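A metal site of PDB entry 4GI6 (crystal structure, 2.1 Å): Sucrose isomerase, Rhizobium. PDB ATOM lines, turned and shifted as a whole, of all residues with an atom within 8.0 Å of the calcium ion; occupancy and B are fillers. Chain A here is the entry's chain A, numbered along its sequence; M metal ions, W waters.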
ATOM      1  N   PRO A  17     -30.619 -19.623  27.103  1.00  0.00           N
ATOM      2  CA  PRO A  17     -29.492 -20.461  26.647  1.00  0.00           C
ATOM      3  C   PRO A  17     -29.021 -20.092  25.250  1.00  0.00           C
ATOM      4  O   PRO A  17     -27.839 -20.084  24.996  1.00  0.00           O
ATOM      5  CB  PRO A  17     -30.052 -21.897  26.677  1.00  0.00           C
ATOM      6  CG  PRO A  17     -31.264 -21.833  27.596  1.00  0.00           C
ATOM      7  CD  PRO A  17     -31.805 -20.435  27.473  1.00  0.00           C
ATOM      8  N   ARG A  18     -29.969 -19.801  24.361  1.00  0.00           N
ATOM      9  CA  ARG A  18     -29.693 -19.290  23.029  1.00  0.00           C
ATOM     10  C   ARG A  18     -28.676 -18.116  22.980  1.00  0.00           C
ATOM     11  O   ARG A  18     -27.950 -17.994  21.998  1.00  0.00           O
ATOM     12  CB  ARG A  18     -31.017 -18.819  22.448  1.00  0.00           C
ATOM     13  CG  ARG A  18     -30.981 -18.552  20.982  1.00  0.00           C
ATOM     14  CD  ARG A  18     -32.371 -18.285  20.411  1.00  0.00           C
ATOM     15  NE  ARG A  18     -32.213 -18.034  18.984  1.00  0.00           N
ATOM     16  CZ  ARG A  18     -32.285 -18.972  18.041  1.00  0.00           C
ATOM     17  NH1 ARG A  18     -32.561 -20.252  18.346  1.00  0.00           N
ATOM     18  NH2 ARG A  18     -32.094 -18.639  16.770  1.00  0.00           N
ATOM     19  N   LYS A  21     -24.008 -18.660  26.137  1.00  0.00           N
ATOM     20  CA  LYS A  21     -22.639 -19.028  25.729  1.00  0.00           C
ATOM     21  C   LYS A  21     -22.556 -20.166  24.701  1.00  0.00           C
ATOM     22  O   LYS A  21     -23.036 -21.269  24.964  1.00  0.00           O
ATOM     23  CB  LYS A  21     -21.789 -19.352  26.992  1.00  0.00           C
ATOM     24  CG  LYS A  21     -20.317 -19.681  26.743  1.00  0.00           C
ATOM     25  CD  LYS A  21     -19.578 -18.491  26.146  1.00  0.00           C
ATOM     26  CE  LYS A  21     -18.463 -18.981  25.233  1.00  0.00           C
ATOM     27  NZ  LYS A  21     -17.196 -19.125  25.981  1.00  0.00           N
ATOM     28  N   ASP A  22     -21.949 -19.883  23.538  1.00  0.00           N
ATOM     29  CA  ASP A  22     -21.748 -20.857  22.444  1.00  0.00           C
ATOM     30  C   ASP A  22     -20.414 -21.594  22.632  1.00  0.00           C
ATOM     31  O   ASP A  22     -19.409 -20.970  22.974  1.00  0.00           O
ATOM     32  CB  ASP A  22     -21.754 -20.107  21.089  1.00  0.00           C
ATOM     33  CG  ASP A  22     -21.593 -21.012  19.867  1.00  0.00           C
ATOM     34  OD1 ASP A  22     -21.690 -22.249  19.920  1.00  0.00           O
ATOM     35  OD2 ASP A  22     -21.373 -20.459  18.792  1.00  0.00           O
ATOM     36  N   THR A  23     -20.396 -22.905  22.407  1.00  0.00           N
ATOM     37  CA  THR A  23     -19.118 -23.687  22.508  1.00  0.00           C
ATOM     38  C   THR A  23     -18.704 -24.392  21.214  1.00  0.00           C
ATOM     39  O   THR A  23     -17.684 -25.090  21.170  1.00  0.00           O
ATOM     40  CB  THR A  23     -19.182 -24.730  23.642  1.00  0.00           C
ATOM     41  OG1 THR A  23     -20.417 -25.475  23.554  1.00  0.00           O
ATOM     42  CG2 THR A  23     -19.092 -24.043  25.026  1.00  0.00           C
ATOM     43  N   ASN A  24     -19.489 -24.262  20.150  1.00  0.00           N
ATOM     44  CA  ASN A  24     -19.115 -24.906  18.914  1.00  0.00           C
ATOM     45  C   ASN A  24     -19.227 -24.010  17.700  1.00  0.00           C
ATOM     46  O   ASN A  24     -19.427 -24.504  16.613  1.00  0.00           O
ATOM     47  CB  ASN A  24     -19.944 -26.174  18.710  1.00  0.00           C
ATOM     48  CG  ASN A  24     -21.413 -25.885  18.453  1.00  0.00           C
ATOM     49  OD1 ASN A  24     -21.889 -24.787  18.694  1.00  0.00           O
ATOM     50  ND2 ASN A  24     -22.124 -26.861  17.913  1.00  0.00           N
ATOM     51  N   GLY A  25     -19.142 -22.699  17.883  1.00  0.00           N
ATOM     52  CA  GLY A  25     -19.139 -21.775  16.738  1.00  0.00           C
ATOM     53  C   GLY A  25     -20.325 -21.724  15.764  1.00  0.00           C
ATOM     54  O   GLY A  25     -20.147 -21.303  14.629  1.00  0.00           O
ATOM     55  N   ASP A  26     -21.522 -22.112  16.184  1.00  0.00           N
ATOM     56  CA  ASP A  26     -22.655 -21.983  15.287  1.00  0.00           C
ATOM     57  C   ASP A  26     -23.453 -20.708  15.563  1.00  0.00           C
ATOM     58  O   ASP A  26     -24.467 -20.419  14.895  1.00  0.00           O
ATOM     59  CB  ASP A  26     -23.532 -23.245  15.369  1.00  0.00           C
ATOM     60  CG  ASP A  26     -24.389 -23.314  16.665  1.00  0.00           C
ATOM     61  OD1 ASP A  26     -24.090 -22.641  17.681  1.00  0.00           O
ATOM     62  OD2 ASP A  26     -25.412 -24.054  16.643  1.00  0.00           O
ATOM     63  N   GLY A  27     -22.993 -19.936  16.549  1.00  0.00           N
ATOM     64  CA  GLY A  27     -23.606 -18.639  16.882  1.00  0.00           C
ATOM     65  C   GLY A  27     -24.826 -18.736  17.812  1.00  0.00           C
ATOM     66  O   GLY A  27     -25.511 -17.718  18.067  1.00  0.00           O
ATOM     67  N   ILE A  28     -25.088 -19.935  18.318  1.00  0.00           N
ATOM     68  CA  ILE A  28     -26.232 -20.177  19.211  1.00  0.00           C
ATOM     69  C   ILE A  28     -25.698 -20.731  20.560  1.00  0.00           C
ATOM     70  O   ILE A  28     -24.865 -21.629  20.586  1.00  0.00           O
ATOM     71  CB  ILE A  28     -27.279 -21.102  18.549  1.00  0.00           C
ATOM     72  CG1 ILE A  28     -27.961 -20.371  17.369  1.00  0.00           C
ATOM     73  CG2 ILE A  28     -28.355 -21.561  19.544  1.00  0.00           C
ATOM     74  CD1 ILE A  28     -28.778 -21.258  16.437  1.00  0.00           C
ATOM     75  N   GLY A  29     -26.152 -20.156  21.679  1.00  0.00           N
ATOM     76  CA  GLY A  29     -25.710 -20.648  22.979  1.00  0.00           C
ATOM     77  C   GLY A  29     -26.118 -22.105  23.139  1.00  0.00           C
ATOM     78  O   GLY A  29     -27.020 -22.602  22.460  1.00  0.00           O
ATOM     79  N   ASP A  30     -25.452 -22.806  24.038  1.00  0.00           N
ATOM     80  CA  ASP A  30     -25.773 -24.222  24.234  1.00  0.00           C
ATOM     81  C   ASP A  30     -25.600 -24.599  25.695  1.00  0.00           C
ATOM     82  O   ASP A  30     -25.092 -23.814  26.509  1.00  0.00           O
ATOM     83  CB  ASP A  30     -24.890 -25.087  23.298  1.00  0.00           C
ATOM     84  CG  ASP A  30     -23.465 -24.586  23.229  1.00  0.00           C
ATOM     85  OD1 ASP A  30     -22.741 -24.621  24.255  1.00  0.00           O
ATOM     86  OD2 ASP A  30     -23.051 -24.104  22.166  1.00  0.00           O
ATOM     87  N   PHE A  31     -25.963 -25.844  26.009  1.00  0.00           N
ATOM     88  CA  PHE A  31     -25.831 -26.396  27.340  1.00  0.00           C
ATOM     89  C   PHE A  31     -24.408 -26.438  27.799  1.00  0.00           C
ATOM     90  O   PHE A  31     -24.142 -26.096  28.953  1.00  0.00           O
ATOM     91  CB  PHE A  31     -26.365 -27.837  27.357  1.00  0.00           C
ATOM     92  CG  PHE A  31     -27.863 -27.921  27.410  1.00  0.00           C
ATOM     93  CD1 PHE A  31     -28.598 -27.055  28.190  1.00  0.00           C
ATOM     94  CD2 PHE A  31     -28.522 -28.884  26.661  1.00  0.00           C
ATOM     95  CE1 PHE A  31     -29.975 -27.161  28.234  1.00  0.00           C
ATOM     96  CE2 PHE A  31     -29.895 -28.987  26.692  1.00  0.00           C
ATOM     97  CZ  PHE A  31     -30.625 -28.124  27.489  1.00  0.00           C
ATOM     98  N   LYS A  32     -23.482 -26.846  26.918  1.00  0.00           N
ATOM     99  CA  LYS A  32     -22.066 -26.931  27.303  1.00  0.00           C
ATOM    100  C   LYS A  32     -21.549 -25.521  27.647  1.00  0.00           C
ATOM    101  O   LYS A  32     -20.743 -25.355  28.569  1.00  0.00           O
ATOM    102  CB  LYS A  32     -21.256 -27.571  26.195  1.00  0.00           C
ATOM    103  CG  LYS A  32     -19.903 -28.121  26.600  1.00  0.00           C
ATOM    104  N   GLY A  33     -22.045 -24.494  26.939  1.00  0.00           N
ATOM    105  CA  GLY A  33     -21.687 -23.121  27.295  1.00  0.00           C
ATOM    106  C   GLY A  33     -22.230 -22.735  28.674  1.00  0.00           C
ATOM    107  O   GLY A  33     -21.510 -22.172  29.500  1.00  0.00           O
ATOM    108  N   LYS A  74     -32.053 -29.633  19.672  1.00  0.00           N
ATOM    109  CA  LYS A  74     -30.868 -29.999  18.884  1.00  0.00           C
ATOM    110  C   LYS A  74     -29.702 -28.995  19.019  1.00  0.00           C
ATOM    111  O   LYS A  74     -28.577 -29.389  19.275  1.00  0.00           O
ATOM    112  CB  LYS A  74     -31.257 -30.198  17.396  1.00  0.00           C
ATOM    113  N   GLU A  75     -30.011 -27.707  18.885  1.00  0.00           N
ATOM    114  CA  GLU A  75     -29.040 -26.625  19.040  1.00  0.00           C
ATOM    115  C   GLU A  75     -28.330 -26.574  20.421  1.00  0.00           C
ATOM    116  O   GLU A  75     -27.159 -26.188  20.503  1.00  0.00           O
ATOM    117  CB  GLU A  75     -29.719 -25.274  18.765  1.00  0.00           C
ATOM    118  CG  GLU A  75     -30.007 -24.981  17.302  1.00  0.00           C
ATOM    119  CD  GLU A  75     -31.282 -25.618  16.767  1.00  0.00           C
ATOM    120  OE1 GLU A  75     -32.002 -26.342  17.482  1.00  0.00           O
ATOM    121  OE2 GLU A  75     -31.581 -25.350  15.598  1.00  0.00           O
ATOM    122  N   TYR A  76     -29.037 -26.945  21.485  1.00  0.00           N
ATOM    123  CA  TYR A  76     -28.422 -26.907  22.832  1.00  0.00           C
ATOM    124  C   TYR A  76     -27.577 -28.131  23.209  1.00  0.00           C
ATOM    125  O   TYR A  76     -26.691 -28.014  24.053  1.00  0.00           O
ATOM    126  CB  TYR A  76     -29.463 -26.639  23.940  1.00  0.00           C
ATOM    127  CG  TYR A  76     -30.269 -25.381  23.742  1.00  0.00           C
ATOM    128  CD1 TYR A  76     -29.814 -24.367  22.897  1.00  0.00           C
ATOM    129  CD2 TYR A  76     -31.486 -25.183  24.436  1.00  0.00           C
ATOM    130  CE1 TYR A  76     -30.556 -23.226  22.701  1.00  0.00           C
ATOM    131  CE2 TYR A  76     -32.231 -24.023  24.251  1.00  0.00           C
ATOM    132  CZ  TYR A  76     -31.764 -23.050  23.364  1.00  0.00           C
ATOM    133  OH  TYR A  76     -32.486 -21.891  23.149  1.00  0.00           O
ATOM    134  N   GLY A  77     -27.853 -29.283  22.620  1.00  0.00           N
ATOM    135  CA  GLY A  77     -27.059 -30.459  22.948  1.00  0.00           C
ATOM    136  C   GLY A  77     -27.951 -31.660  23.082  1.00  0.00           C
ATOM    137  O   GLY A  77     -29.039 -31.681  22.524  1.00  0.00           O
ATOM    138  N   PHE A 431     -18.789 -14.330  23.231  1.00  0.00           N
ATOM    139  CA  PHE A 431     -19.988 -15.161  23.141  1.00  0.00           C
ATOM    140  C   PHE A 431     -19.795 -16.370  22.198  1.00  0.00           C
ATOM    141  O   PHE A 431     -20.238 -17.466  22.533  1.00  0.00           O
ATOM    142  CB  PHE A 431     -21.204 -14.352  22.697  1.00  0.00           C
ATOM    143  CG  PHE A 431     -22.370 -15.202  22.273  1.00  0.00           C
ATOM    144  CD1 PHE A 431     -23.087 -15.945  23.220  1.00  0.00           C
ATOM    145  CD2 PHE A 431     -22.724 -15.310  20.936  1.00  0.00           C
ATOM    146  CE1 PHE A 431     -24.143 -16.766  22.825  1.00  0.00           C
ATOM    147  CE2 PHE A 431     -23.789 -16.116  20.540  1.00  0.00           C
ATOM    148  CZ  PHE A 431     -24.497 -16.846  21.493  1.00  0.00           C
ATOM    149  N   THR A 432     -19.157 -16.176  21.046  1.00  0.00           N
ATOM    150  CA  THR A 432     -19.041 -17.219  20.012  1.00  0.00           C
ATOM    151  C   THR A 432     -17.781 -16.978  19.182  1.00  0.00           C
ATOM    152  O   THR A 432     -17.283 -15.840  19.128  1.00  0.00           O
ATOM    153  CB  THR A 432     -20.237 -17.183  19.007  1.00  0.00           C
ATOM    154  OG1 THR A 432     -20.074 -18.189  17.999  1.00  0.00           O
ATOM    155  CG2 THR A 432     -20.318 -15.838  18.310  1.00  0.00           C
HETATM  156 CA    CA M   1     -23.723 -23.579  19.850  1.00  0.00          CA
HETATM  157  O   HOH W   1     -25.893 -24.345  19.228  1.00  0.00           O
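The backbone NH (N) of Asp 30 sits at hydrogen-bond distance from the backbone carbonyl oxygen (O) of Lys 21 (3.0 Å). The backbone NH (N) of Gly 33 lies within hydrogen-bond range of the side-chain carboxylate (OD1) of Asp 30 (2.8 Å). OD1 of Asp 30 sits at hydrogen-bond distance from OG1 of Thr 23 (2.6 Å). The side-chain carboxylate of Asp 22 is in hydrogen-bond range of the backbone NH of Gly 27, 2.8 Å away. The side-chain carboxylate (OD2) of Asp 22 lies within hydrogen-bond range of the backbone NH (N) of Gly 25. The side-chain carboxylate of Asp 22 lies within hydrogen-bond range of the side-chain hydroxyl of Thr 432 (2.7 Å). The backbone NH (N) of Asp 22 is in hydrogen-bond range of the backbone carbonyl oxygen (O) of Phe 431, 3.1 Å away.
Five residues have an atom within 4 Å of the calcium ion: Asp 22, Asn 24, Asp 26, Ile 28 and Asp 30. The nearest printed residue that does not touch the calcium ion is Thr 23 (4.2 Å).
The calcium ion is bound by O of Ile 28 (2.4 Å). The calcium ion is bound by water W1 (2.4 Å). The side-chain carboxylate (OD1) of Asp 26 binds the calcium ion, at 2.4 Å. The side-chain carboxylate (OD1) of Asp 22 is bound to the calcium ion, at 2.4 Å. The calcium ion is bound by the side-chain carboxylate (OD2) of Asp 30 (2.5 Å). The side-chain amide oxygen (OD1) of Asn 24 is bound to the calcium ion, at 2.5 Å. The calcium ion has six donor atoms within binding distance.
Water W1 bridges the backbone carbonyl oxygen of Glu 75 (2.6 Å) and the side-chain carboxylate of Asp 26 (2.6 Å).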
